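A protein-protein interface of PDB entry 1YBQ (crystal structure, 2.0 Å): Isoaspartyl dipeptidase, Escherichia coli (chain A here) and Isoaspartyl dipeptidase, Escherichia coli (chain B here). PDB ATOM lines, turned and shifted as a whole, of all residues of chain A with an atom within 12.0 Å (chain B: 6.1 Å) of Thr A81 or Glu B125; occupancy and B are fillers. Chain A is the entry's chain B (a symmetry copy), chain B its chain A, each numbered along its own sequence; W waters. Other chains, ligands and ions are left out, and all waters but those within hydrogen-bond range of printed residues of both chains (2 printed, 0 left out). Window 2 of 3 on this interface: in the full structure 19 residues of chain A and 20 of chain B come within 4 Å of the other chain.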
ATOM      1  N   ILE A  72     -19.002 -22.966  37.301  1.00  0.00           N
ATOM      2  CA  ILE A  72     -19.704 -24.041  36.630  1.00  0.00           C
ATOM      3  C   ILE A  72     -20.732 -23.533  35.668  1.00  0.00           C
ATOM      4  O   ILE A  72     -21.422 -24.312  35.020  1.00  0.00           O
ATOM      5  CB  ILE A  72     -20.361 -25.048  37.576  1.00  0.00           C
ATOM      6  CG1 ILE A  72     -21.265 -24.397  38.613  1.00  0.00           C
ATOM      7  CG2 ILE A  72     -19.316 -25.938  38.227  1.00  0.00           C
ATOM      8  CD1 ILE A  72     -22.164 -25.450  39.318  1.00  0.00           C
ATOM      9  N   GLY A  73     -20.808 -22.220  35.588  1.00  0.00           N
ATOM     10  CA  GLY A  73     -21.779 -21.603  34.735  1.00  0.00           C
ATOM     11  C   GLY A  73     -22.771 -20.926  35.677  1.00  0.00           C
ATOM     12  O   GLY A  73     -22.750 -21.189  36.865  1.00  0.00           O
ATOM     13  N   GLY A  74     -23.600 -20.046  35.132  1.00  0.00           N
ATOM     14  CA  GLY A  74     -24.587 -19.274  35.864  1.00  0.00           C
ATOM     15  C   GLY A  74     -25.762 -19.021  34.949  1.00  0.00           C
ATOM     16  O   GLY A  74     -26.180 -19.908  34.181  1.00  0.00           O
ATOM     17  N   GLY A  75     -26.268 -17.791  35.046  1.00  0.00           N
ATOM     18  CA  GLY A  75     -27.389 -17.351  34.256  1.00  0.00           C
ATOM     19  C   GLY A  75     -28.637 -18.156  34.611  1.00  0.00           C
ATOM     20  O   GLY A  75     -28.803 -18.682  35.742  1.00  0.00           O
ATOM     21  N   GLY A  76     -29.515 -18.234  33.600  1.00  0.00           N
ATOM     22  CA  GLY A  76     -30.786 -18.961  33.664  1.00  0.00           C
ATOM     23  C   GLY A  76     -31.990 -18.082  33.981  1.00  0.00           C
ATOM     24  O   GLY A  76     -33.102 -18.607  34.102  1.00  0.00           O
ATOM     25  N   GLU A  77     -31.772 -16.751  34.135  1.00  0.00           N
ATOM     26  CA  GLU A  77     -32.855 -15.792  34.442  1.00  0.00           C
ATOM     27  C   GLU A  77     -33.926 -15.671  33.341  1.00  0.00           C
ATOM     28  O   GLU A  77     -34.979 -15.048  33.499  1.00  0.00           O
ATOM     29  CB  GLU A  77     -32.314 -14.372  34.669  1.00  0.00           C
ATOM     30  CG  GLU A  77     -31.540 -14.217  35.979  1.00  0.00           C
ATOM     31  CD  GLU A  77     -30.051 -14.407  35.886  1.00  0.00           C
ATOM     32  OE1 GLU A  77     -29.463 -15.056  35.015  1.00  0.00           O
ATOM     33  OE2 GLU A  77     -29.485 -13.830  36.910  1.00  0.00           O
ATOM     34  N   ALA A  78     -33.652 -16.218  32.176  1.00  0.00           N
ATOM     35  CA  ALA A  78     -34.623 -16.152  31.106  1.00  0.00           C
ATOM     36  C   ALA A  78     -34.832 -17.557  30.565  1.00  0.00           C
ATOM     37  O   ALA A  78     -34.887 -17.784  29.358  1.00  0.00           O
ATOM     38  CB  ALA A  78     -34.097 -15.273  29.993  1.00  0.00           C
ATOM     39  N   GLY A  79     -34.878 -18.503  31.476  1.00  0.00           N
ATOM     40  CA  GLY A  79     -35.065 -19.881  31.074  1.00  0.00           C
ATOM     41  C   GLY A  79     -33.741 -20.562  30.843  1.00  0.00           C
ATOM     42  O   GLY A  79     -32.682 -19.917  30.796  1.00  0.00           O
ATOM     43  N   PRO A  80     -33.868 -21.875  30.640  1.00  0.00           N
ATOM     44  CA  PRO A  80     -32.815 -22.848  30.443  1.00  0.00           C
ATOM     45  C   PRO A  80     -31.814 -22.555  29.355  1.00  0.00           C
ATOM     46  O   PRO A  80     -30.657 -22.959  29.459  1.00  0.00           O
ATOM     47  CB  PRO A  80     -33.493 -24.174  30.120  1.00  0.00           C
ATOM     48  CG  PRO A  80     -34.971 -23.972  30.357  1.00  0.00           C
ATOM     49  CD  PRO A  80     -35.203 -22.496  30.625  1.00  0.00           C
ATOM     50  N   THR A  81     -32.239 -21.901  28.291  1.00  0.00           N
ATOM     51  CA  THR A  81     -31.253 -21.625  27.261  1.00  0.00           C
ATOM     52  C   THR A  81     -30.271 -20.548  27.741  1.00  0.00           C
ATOM     53  O   THR A  81     -29.211 -20.409  27.175  1.00  0.00           O
ATOM     54  CB  THR A  81     -31.907 -21.150  25.977  1.00  0.00           C
ATOM     55  OG1 THR A  81     -32.337 -19.811  26.219  1.00  0.00           O
ATOM     56  CG2 THR A  81     -33.051 -22.095  25.571  1.00  0.00           C
ATOM     57  N   THR A  82     -30.590 -19.796  28.791  1.00  0.00           N
ATOM     58  CA  THR A  82     -29.663 -18.780  29.236  1.00  0.00           C
ATOM     59  C   THR A  82     -28.753 -19.261  30.344  1.00  0.00           C
ATOM     60  O   THR A  82     -28.160 -18.460  31.069  1.00  0.00           O
ATOM     61  CB  THR A  82     -30.351 -17.467  29.611  1.00  0.00           C
ATOM     62  OG1 THR A  82     -31.174 -17.709  30.731  1.00  0.00           O
ATOM     63  CG2 THR A  82     -31.217 -17.014  28.460  1.00  0.00           C
ATOM     64  N   ARG A  83     -28.614 -20.565  30.494  1.00  0.00           N
ATOM     65  CA  ARG A  83     -27.673 -21.081  31.478  1.00  0.00           C
ATOM     66  C   ARG A  83     -26.294 -20.987  30.824  1.00  0.00           C
ATOM     67  O   ARG A  83     -26.048 -21.642  29.795  1.00  0.00           O
ATOM     68  CB  ARG A  83     -27.950 -22.542  31.796  1.00  0.00           C
ATOM     69  CG  ARG A  83     -29.229 -22.584  32.614  1.00  0.00           C
ATOM     70  CD  ARG A  83     -29.755 -23.991  32.635  1.00  0.00           C
ATOM     71  NE  ARG A  83     -29.039 -24.802  33.609  1.00  0.00           N
ATOM     72  CZ  ARG A  83     -28.188 -25.796  33.323  1.00  0.00           C
ATOM     73  NH1 ARG A  83     -27.887 -26.148  32.068  1.00  0.00           N
ATOM     74  NH2 ARG A  83     -27.620 -26.469  34.318  1.00  0.00           N
ATOM     75  N   THR A  84     -25.396 -20.181  31.398  1.00  0.00           N
ATOM     76  CA  THR A  84     -24.076 -19.983  30.848  1.00  0.00           C
ATOM     77  C   THR A  84     -23.143 -21.181  31.035  1.00  0.00           C
ATOM     78  O   THR A  84     -23.314 -22.030  31.875  1.00  0.00           O
ATOM     79  CB  THR A  84     -23.492 -18.663  31.322  1.00  0.00           C
ATOM     80  OG1 THR A  84     -23.213 -18.861  32.644  1.00  0.00           O
ATOM     81  CG2 THR A  84     -24.559 -17.572  31.342  1.00  0.00           C
ATOM     82  N   PRO A  85     -22.134 -21.277  30.201  1.00  0.00           N
ATOM     83  CA  PRO A  85     -21.199 -22.400  30.246  1.00  0.00           C
ATOM     84  C   PRO A  85     -20.132 -22.302  31.343  1.00  0.00           C
ATOM     85  O   PRO A  85     -19.919 -21.237  31.987  1.00  0.00           O
ATOM     86  CB  PRO A  85     -20.570 -22.426  28.859  1.00  0.00           C
ATOM     87  CG  PRO A  85     -21.059 -21.179  28.131  1.00  0.00           C
ATOM     88  CD  PRO A  85     -21.786 -20.311  29.136  1.00  0.00           C
ATOM     89  N   GLU A  86     -19.485 -23.448  31.605  1.00  0.00           N
ATOM     90  CA  GLU A  86     -18.458 -23.480  32.653  1.00  0.00           C
ATOM     91  C   GLU A  86     -17.246 -22.708  32.200  1.00  0.00           C
ATOM     92  O   GLU A  86     -17.059 -22.487  31.007  1.00  0.00           O
ATOM     93  CB  GLU A  86     -17.999 -24.907  33.007  1.00  0.00           C
ATOM     94  CG  GLU A  86     -17.389 -25.662  31.814  1.00  0.00           C
ATOM     95  CD  GLU A  86     -17.002 -27.078  32.190  1.00  0.00           C
ATOM     96  OE1 GLU A  86     -16.358 -27.309  33.167  1.00  0.00           O
ATOM     97  OE2 GLU A  86     -17.397 -28.030  31.383  1.00  0.00           O
ATOM     98  N   ASP A 107     -29.549 -19.146  40.108  1.00  0.00           N
ATOM     99  CA  ASP A 107     -30.029 -20.509  40.048  1.00  0.00           C
ATOM    100  C   ASP A 107     -29.279 -21.467  40.960  1.00  0.00           C
ATOM    101  O   ASP A 107     -28.074 -21.703  40.831  1.00  0.00           O
ATOM    102  CB  ASP A 107     -29.950 -20.953  38.572  1.00  0.00           C
ATOM    103  CG  ASP A 107     -30.371 -22.383  38.338  1.00  0.00           C
ATOM    104  OD1 ASP A 107     -30.803 -23.129  39.177  1.00  0.00           O
ATOM    105  OD2 ASP A 107     -30.168 -22.759  37.116  1.00  0.00           O
ATOM    106  N   SER A 110     -30.772 -25.920  39.253  1.00  0.00           N
ATOM    107  CA  SER A 110     -30.107 -26.695  38.226  1.00  0.00           C
ATOM    108  C   SER A 110     -28.619 -26.600  38.464  1.00  0.00           C
ATOM    109  O   SER A 110     -27.841 -27.198  37.722  1.00  0.00           O
ATOM    110  CB  SER A 110     -30.441 -26.184  36.836  1.00  0.00           C
ATOM    111  OG  SER A 110     -29.617 -25.052  36.586  1.00  0.00           O
ATOM    112  N   ARG A 111     -28.242 -25.804  39.493  1.00  0.00           N
ATOM    113  CA  ARG A 111     -26.831 -25.570  39.897  1.00  0.00           C
ATOM    114  C   ARG A 111     -26.659 -26.085  41.316  1.00  0.00           C
ATOM    115  O   ARG A 111     -27.500 -25.784  42.166  1.00  0.00           O
ATOM    116  CB  ARG A 111     -26.390 -24.104  39.834  1.00  0.00           C
ATOM    117  CG  ARG A 111     -26.578 -23.447  38.458  1.00  0.00           C
ATOM    118  CD  ARG A 111     -25.977 -24.241  37.272  1.00  0.00           C
ATOM    119  NE  ARG A 111     -25.891 -23.384  36.061  1.00  0.00           N
ATOM    120  CZ  ARG A 111     -25.184 -23.614  34.955  1.00  0.00           C
ATOM    121  NH1 ARG A 111     -24.462 -24.730  34.790  1.00  0.00           N
ATOM    122  NH2 ARG A 111     -25.221 -22.697  33.979  1.00  0.00           N
ATOM    123  N   ASN A 287     -18.344 -15.347  33.642  1.00  0.00           N
ATOM    124  CA  ASN A 287     -19.252 -16.451  33.328  1.00  0.00           C
ATOM    125  C   ASN A 287     -20.629 -16.293  33.862  1.00  0.00           C
ATOM    126  O   ASN A 287     -21.482 -17.132  33.647  1.00  0.00           O
ATOM    127  CB  ASN A 287     -18.734 -17.890  33.510  1.00  0.00           C
ATOM    128  CG  ASN A 287     -18.063 -18.323  32.242  1.00  0.00           C
ATOM    129  OD1 ASN A 287     -17.056 -17.711  31.863  1.00  0.00           O
ATOM    130  ND2 ASN A 287     -18.658 -19.298  31.566  1.00  0.00           N
ATOM    131  N   GLY A 288     -20.829 -15.190  34.571  1.00  0.00           N
ATOM    132  CA  GLY A 288     -22.142 -14.928  35.078  1.00  0.00           C
ATOM    133  C   GLY A 288     -22.976 -14.211  34.022  1.00  0.00           C
ATOM    134  O   GLY A 288     -22.446 -13.561  33.114  1.00  0.00           O
ATOM    135  N   SER A 289     -24.296 -14.321  34.125  1.00  0.00           N
ATOM    136  CA  SER A 289     -25.145 -13.616  33.197  1.00  0.00           C
ATOM    137  C   SER A 289     -25.188 -12.139  33.637  1.00  0.00           C
ATOM    138  O   SER A 289     -24.980 -11.805  34.829  1.00  0.00           O
ATOM    139  CB  SER A 289     -26.552 -14.195  33.154  1.00  0.00           C
ATOM    140  OG  SER A 289     -27.179 -14.000  34.404  1.00  0.00           O
ATOM    141  N   GLN A 290     -25.433 -11.274  32.654  1.00  0.00           N
ATOM    142  CA  GLN A 290     -25.548  -9.831  32.837  1.00  0.00           C
ATOM    143  C   GLN A 290     -26.928  -9.435  32.350  1.00  0.00           C
ATOM    144  O   GLN A 290     -27.129  -8.926  31.233  1.00  0.00           O
ATOM    145  CB  GLN A 290     -24.412  -9.021  32.154  1.00  0.00           C
ATOM    146  CG  GLN A 290     -22.985  -9.378  32.648  1.00  0.00           C
ATOM    147  CD  GLN A 290     -21.902  -8.686  31.869  1.00  0.00           C
ATOM    148  OE1 GLN A 290     -21.525  -7.545  32.183  1.00  0.00           O
ATOM    149  NE2 GLN A 290     -21.367  -9.345  30.809  1.00  0.00           N
ATOM    150  N   PRO A 291     -27.892  -9.757  33.206  1.00  0.00           N
ATOM    151  CA  PRO A 291     -29.272  -9.498  32.872  1.00  0.00           C
ATOM    152  C   PRO A 291     -29.669  -8.104  33.297  1.00  0.00           C
ATOM    153  O   PRO A 291     -29.201  -7.567  34.321  1.00  0.00           O
ATOM    154  CB  PRO A 291     -30.082 -10.529  33.669  1.00  0.00           C
ATOM    155  CG  PRO A 291     -29.199 -10.913  34.846  1.00  0.00           C
ATOM    156  CD  PRO A 291     -27.784 -10.466  34.513  1.00  0.00           C
ATOM    157  N   LEU A 299     -37.315  -8.804  32.367  1.00  0.00           N
ATOM    158  CA  LEU A 299     -36.031  -8.946  31.691  1.00  0.00           C
ATOM    159  C   LEU A 299     -36.039  -8.370  30.272  1.00  0.00           C
ATOM    160  O   LEU A 299     -36.754  -8.838  29.383  1.00  0.00           O
ATOM    161  CB  LEU A 299     -35.475 -10.394  31.718  1.00  0.00           C
ATOM    162  CG  LEU A 299     -34.006 -10.497  31.297  1.00  0.00           C
ATOM    163  CD1 LEU A 299     -33.280 -11.565  32.114  1.00  0.00           C
ATOM    164  CD2 LEU A 299     -33.884 -10.817  29.814  1.00  0.00           C
ATOM    165  N   HIS A 301     -32.749  -7.397  28.688  1.00  0.00           N
ATOM    166  CA  HIS A 301     -31.513  -7.863  28.084  1.00  0.00           C
ATOM    167  C   HIS A 301     -30.670  -8.834  28.981  1.00  0.00           C
ATOM    168  O   HIS A 301     -30.586  -8.705  30.220  1.00  0.00           O
ATOM    169  CB  HIS A 301     -30.707  -6.582  27.654  1.00  0.00           C
ATOM    170  CG  HIS A 301     -29.295  -6.839  27.241  1.00  0.00           C
ATOM    171  ND1 HIS A 301     -28.231  -6.684  28.123  1.00  0.00           N
ATOM    172  CD2 HIS A 301     -28.782  -7.273  26.058  1.00  0.00           C
ATOM    173  CE1 HIS A 301     -27.117  -7.028  27.475  1.00  0.00           C
ATOM    174  NE2 HIS A 301     -27.417  -7.391  26.227  1.00  0.00           N
ATOM    175  N   ILE A 302     -30.017  -9.825  28.338  1.00  0.00           N
ATOM    176  CA  ILE A 302     -29.123 -10.782  29.010  1.00  0.00           C
ATOM    177  C   ILE A 302     -27.823 -11.073  28.210  1.00  0.00           C
ATOM    178  O   ILE A 302     -27.818 -11.243  26.988  1.00  0.00           O
ATOM    179  CB  ILE A 302     -29.812 -12.028  29.621  1.00  0.00           C
ATOM    180  CG1 ILE A 302     -28.979 -12.658  30.756  1.00  0.00           C
ATOM    181  CG2 ILE A 302     -30.158 -13.055  28.549  1.00  0.00           C
ATOM    182  CD1 ILE A 302     -29.400 -14.066  31.174  1.00  0.00           C
ATOM    183  N   GLY A 303     -26.694 -11.111  28.921  1.00  0.00           N
ATOM    184  CA  GLY A 303     -25.377 -11.420  28.353  1.00  0.00           C
ATOM    185  C   GLY A 303     -24.489 -12.196  29.356  1.00  0.00           C
ATOM    186  O   GLY A 303     -24.923 -12.467  30.483  1.00  0.00           O
ATOM    187  N   VAL A 304     -23.245 -12.547  28.958  1.00  0.00           N
ATOM    188  CA  VAL A 304     -22.269 -13.232  29.818  1.00  0.00           C
ATOM    189  C   VAL A 304     -20.994 -12.402  30.001  1.00  0.00           C
ATOM    190  O   VAL A 304     -20.424 -11.810  29.073  1.00  0.00           O
ATOM    191  CB  VAL A 304     -22.002 -14.731  29.568  1.00  0.00           C
ATOM    192  CG1 VAL A 304     -21.138 -14.941  28.338  1.00  0.00           C
ATOM    193  CG2 VAL A 304     -21.262 -15.355  30.746  1.00  0.00           C
ATOM    194  N   ALA B 118     -32.888 -29.434  33.025  1.00  0.00           N
ATOM    195  CA  ALA B 118     -32.841 -28.060  32.499  1.00  0.00           C
ATOM    196  C   ALA B 118     -32.241 -27.994  31.086  1.00  0.00           C
ATOM    197  O   ALA B 118     -32.673 -27.259  30.183  1.00  0.00           O
ATOM    198  CB  ALA B 118     -32.052 -27.175  33.474  1.00  0.00           C
ATOM    199  N   THR B 120     -32.218 -30.431  28.916  1.00  0.00           N
ATOM    200  CA  THR B 120     -33.180 -31.085  28.013  1.00  0.00           C
ATOM    201  C   THR B 120     -34.174 -30.061  27.504  1.00  0.00           C
ATOM    202  O   THR B 120     -34.491 -29.993  26.326  1.00  0.00           O
ATOM    203  CB  THR B 120     -33.868 -32.303  28.648  1.00  0.00           C
ATOM    204  OG1 THR B 120     -32.892 -33.292  28.903  1.00  0.00           O
ATOM    205  CG2 THR B 120     -34.823 -32.877  27.628  1.00  0.00           C
ATOM    206  N   ARG B 121     -34.619 -29.207  28.412  1.00  0.00           N
ATOM    207  CA  ARG B 121     -35.559 -28.162  28.081  1.00  0.00           C
ATOM    208  C   ARG B 121     -34.971 -27.097  27.200  1.00  0.00           C
ATOM    209  O   ARG B 121     -35.640 -26.607  26.299  1.00  0.00           O
ATOM    210  CB  ARG B 121     -36.232 -27.575  29.310  1.00  0.00           C
ATOM    211  CG  ARG B 121     -37.060 -28.680  29.993  1.00  0.00           C
ATOM    212  CD  ARG B 121     -37.917 -28.234  31.185  1.00  0.00           C
ATOM    213  NE  ARG B 121     -39.042 -29.138  31.501  1.00  0.00           N
ATOM    214  CZ  ARG B 121     -39.587 -29.234  32.711  1.00  0.00           C
ATOM    215  NH1 ARG B 121     -39.144 -28.506  33.748  1.00  0.00           N
ATOM    216  NH2 ARG B 121     -40.618 -30.051  32.898  1.00  0.00           N
ATOM    217  N   ALA B 122     -33.717 -26.747  27.475  1.00  0.00           N
ATOM    218  CA  ALA B 122     -32.995 -25.738  26.712  1.00  0.00           C
ATOM    219  C   ALA B 122     -32.893 -26.173  25.269  1.00  0.00           C
ATOM    220  O   ALA B 122     -33.112 -25.408  24.329  1.00  0.00           O
ATOM    221  CB  ALA B 122     -31.613 -25.555  27.307  1.00  0.00           C
ATOM    222  N   LEU B 123     -32.596 -27.452  25.099  1.00  0.00           N
ATOM    223  CA  LEU B 123     -32.507 -28.007  23.750  1.00  0.00           C
ATOM    224  C   LEU B 123     -33.846 -28.024  23.008  1.00  0.00           C
ATOM    225  O   LEU B 123     -33.978 -27.774  21.796  1.00  0.00           O
ATOM    226  CB  LEU B 123     -31.860 -29.399  23.747  1.00  0.00           C
ATOM    227  CG  LEU B 123     -30.386 -29.323  24.076  1.00  0.00           C
ATOM    228  CD1 LEU B 123     -29.847 -30.735  24.132  1.00  0.00           C
ATOM    229  CD2 LEU B 123     -29.630 -28.455  23.062  1.00  0.00           C
ATOM    230  N   ASN B 124     -34.901 -28.330  23.723  1.00  0.00           N
ATOM    231  CA  ASN B 124     -36.132 -28.309  23.000  1.00  0.00           C
ATOM    232  C   ASN B 124     -36.379 -26.871  22.602  1.00  0.00           C
ATOM    233  O   ASN B 124     -36.916 -26.558  21.564  1.00  0.00           O
ATOM    234  CB  ASN B 124     -37.316 -28.752  23.877  1.00  0.00           C
ATOM    235  CG  ASN B 124     -37.326 -30.247  24.046  1.00  0.00           C
ATOM    236  OD1 ASN B 124     -37.381 -30.970  23.069  1.00  0.00           O
ATOM    237  ND2 ASN B 124     -37.152 -30.701  25.274  1.00  0.00           N
ATOM    238  N   GLU B 125     -36.034 -25.964  23.474  1.00  0.00           N
ATOM    239  CA  GLU B 125     -36.318 -24.609  23.163  1.00  0.00           C
ATOM    240  C   GLU B 125     -35.424 -24.040  22.061  1.00  0.00           C
ATOM    241  O   GLU B 125     -35.789 -23.158  21.264  1.00  0.00           O
ATOM    242  CB  GLU B 125     -36.235 -23.888  24.481  1.00  0.00           C
ATOM    243  CG  GLU B 125     -36.755 -22.486  24.326  1.00  0.00           C
ATOM    244  CD  GLU B 125     -36.785 -21.944  25.693  1.00  0.00           C
ATOM    245  OE1 GLU B 125     -36.827 -22.686  26.662  1.00  0.00           O
ATOM    246  OE2 GLU B 125     -36.689 -20.638  25.691  1.00  0.00           O
ATOM    247  N   GLU B 126     -34.243 -24.601  21.964  1.00  0.00           N
ATOM    248  CA  GLU B 126     -33.355 -24.150  20.913  1.00  0.00           C
ATOM    249  C   GLU B 126     -33.775 -24.644  19.515  1.00  0.00           C
ATOM    250  O   GLU B 126     -33.417 -24.033  18.505  1.00  0.00           O
ATOM    251  CB  GLU B 126     -31.859 -24.367  21.210  1.00  0.00           C
ATOM    252  CG  GLU B 126     -31.254 -23.258  22.093  1.00  0.00           C
ATOM    253  CD  GLU B 126     -30.078 -23.746  22.904  1.00  0.00           C
ATOM    254  OE1 GLU B 126     -29.686 -24.908  22.939  1.00  0.00           O
ATOM    255  OE2 GLU B 126     -29.523 -22.781  23.587  1.00  0.00           O
ATOM    256  N   GLY B 127     -34.538 -25.732  19.420  1.00  0.00           N
ATOM    257  CA  GLY B 127     -34.930 -26.137  18.090  1.00  0.00           C
ATOM    258  C   GLY B 127     -35.040 -27.629  17.876  1.00  0.00           C
ATOM    259  O   GLY B 127     -35.714 -28.067  16.940  1.00  0.00           O
ATOM    260  N   ILE B 128     -34.388 -28.428  18.698  1.00  0.00           N
ATOM    261  CA  ILE B 128     -34.562 -29.855  18.455  1.00  0.00           C
ATOM    262  C   ILE B 128     -35.497 -30.480  19.471  1.00  0.00           C
ATOM    263  O   ILE B 128     -36.229 -29.786  20.180  1.00  0.00           O
ATOM    264  CB  ILE B 128     -33.276 -30.636  18.283  1.00  0.00           C
ATOM    265  CG1 ILE B 128     -32.422 -30.403  19.507  1.00  0.00           C
ATOM    266  CG2 ILE B 128     -32.505 -30.220  17.033  1.00  0.00           C
ATOM    267  CD1 ILE B 128     -31.681 -31.665  19.918  1.00  0.00           C
ATOM    268  N   ARG B 371     -37.884 -29.917  13.078  1.00  0.00           N
ATOM    269  CA  ARG B 371     -39.201 -29.342  13.225  1.00  0.00           C
ATOM    270  C   ARG B 371     -39.483 -28.253  12.202  1.00  0.00           C
ATOM    271  O   ARG B 371     -39.972 -27.150  12.504  1.00  0.00           O
ATOM    272  CB  ARG B 371     -39.526 -28.908  14.654  1.00  0.00           C
ATOM    273  CG  ARG B 371     -39.804 -30.117  15.542  1.00  0.00           C
ATOM    274  CD  ARG B 371     -40.370 -29.758  16.904  1.00  0.00           C
ATOM    275  NE  ARG B 371     -39.333 -29.419  17.874  1.00  0.00           N
ATOM    276  CZ  ARG B 371     -39.193 -28.233  18.475  1.00  0.00           C
ATOM    277  NH1 ARG B 371     -40.022 -27.210  18.284  1.00  0.00           N
ATOM    278  NH2 ARG B 371     -38.178 -28.091  19.322  1.00  0.00           N
ATOM    279  N   THR B 386     -27.526 -20.950  22.307  1.00  0.00           N
ATOM    280  CA  THR B 386     -27.509 -19.601  22.865  1.00  0.00           C
ATOM    281  C   THR B 386     -26.107 -19.060  23.174  1.00  0.00           C
ATOM    282  O   THR B 386     -25.846 -17.854  23.033  1.00  0.00           O
ATOM    283  CB  THR B 386     -28.526 -19.433  24.020  1.00  0.00           C
ATOM    284  OG1 THR B 386     -29.811 -19.804  23.550  1.00  0.00           O
ATOM    285  CG2 THR B 386     -28.576 -17.981  24.507  1.00  0.00           C
ATOM    286  N   PHE B 387     -25.207 -19.973  23.579  1.00  0.00           N
ATOM    287  CA  PHE B 387     -23.837 -19.639  23.941  1.00  0.00           C
ATOM    288  C   PHE B 387     -22.739 -20.273  23.122  1.00  0.00           C
ATOM    289  O   PHE B 387     -21.569 -20.144  23.454  1.00  0.00           O
ATOM    290  CB  PHE B 387     -23.572 -19.745  25.442  1.00  0.00           C
ATOM    291  CG  PHE B 387     -24.395 -18.735  26.213  1.00  0.00           C
ATOM    292  CD1 PHE B 387     -25.312 -19.124  27.191  1.00  0.00           C
ATOM    293  CD2 PHE B 387     -24.303 -17.367  25.963  1.00  0.00           C
ATOM    294  CE1 PHE B 387     -26.096 -18.219  27.919  1.00  0.00           C
ATOM    295  CE2 PHE B 387     -25.075 -16.442  26.677  1.00  0.00           C
ATOM    296  CZ  PHE B 387     -25.973 -16.855  27.667  1.00  0.00           C
HETATM  297  O   HOH W   1     -28.222 -22.886  26.012  1.00  0.00           O
HETATM  298  O   HOH W   2     -34.441 -20.104  27.690  1.00  0.00           O
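The backbone NH (N) of Gly A74 sits at hydrogen-bond distance from the side-chain hydroxyl (OG1) of Thr A84 (2.8 Å).
OG1 of Thr A84 lies within hydrogen-bond range of O of Asn A287 (2.6 Å).
The side-chain carboxylate of Glu B126 lies within hydrogen-bond range of the side-chain hydroxyl of Thr B386, at 3.0 Å.
N of Gly A76 lies within hydrogen-bond range of O of Thr A82 (2.9 Å).
The side-chain carboxylate (OD2) of Asp A107 lies within hydrogen-bond range of the side-chain hydroxyl (OG) of Ser A110 (2.4 Å).
NE of Arg A83 lies within hydrogen-bond range of OG of Ser A110, 3.0 Å away.
CB of Pro A80 touches O of Ala B118, 3.2 Å away.
CG of Pro A80 touches CB of Arg B121 (3.96 Å).
Thr A81 touches Glu B125 (CG2 to CD, 3.7 Å).
CB of Thr A81 touches OE2 of Glu B126 (3.7 Å).
CB of Thr B386 touches O of Thr A81, at 3.4 Å.
Thr A82 touches Phe B387.
Ala B118 touches Arg A83 (CB to NE, 3.8 Å).
Thr A84 touches Phe B387 (CG2 to CE1, 3.8 Å).
CG of Pro A85 touches CB of Phe B387, at 3.9 Å.
CB of Ser A110 touches CB of Ala B118 (3.9 Å).
Water W2 lies within hydrogen-bond range of OG1 of Thr A81 (2.6 Å), O of Ala A78 (2.9 Å) and OE2 of Glu B125 (3.1 Å).
Water W1 lies within hydrogen-bond range of the side-chain carboxylate (OE2) of Glu B126 (2.8 Å) and the backbone carbonyl oxygen (O) of Thr A81 (2.9 Å).
Hydrophobic or aromatic side chains of chain B within 4 Å of the printed part of chain A: Ala B118, Ala B122 and Phe B387.
Along chain B the printed residues that touch a printed residue of chain A span positions 118 to 387.
Among the printed residues, no Asp or Glu carboxylate lies within 4 Å of a Lys or Arg side-chain nitrogen of the other chain.
Of chain B, only Ala B122 (3.5 Å), Glu B125 (3.7 Å), Glu B126 (3.7 Å), Thr B386 (3.4 Å) and Phe B387 (3.9 Å) come within 4 Å of Thr A81.
Of chain A, only Thr A81 comes within 4 Å of Glu B125.
No residue of chain A comes within 4 Å of Asn B124.
Glu B126 touches one residue of chain A.
No residue of chain A comes within 4 Å of Gly B127.
Of the printed residues of chain B, Arg A83 touches Ala B118 (3.8 Å) and Phe B387 (3.7 Å).
Of the printed residues of chain A, Phe B387 touches Thr A81 (3.9 Å), Thr A82 (3.7 Å), Arg A83 (3.7 Å), Thr A84 (3.8 Å) and Pro A85 (3.9 Å).
Asp A107 touches none of the printed residues of chain B.
Thr B120 touches none of the printed residues of chain A.
The nearest printed residue of chain B that does not touch Pro A85 is Thr B386 (7.4 Å).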
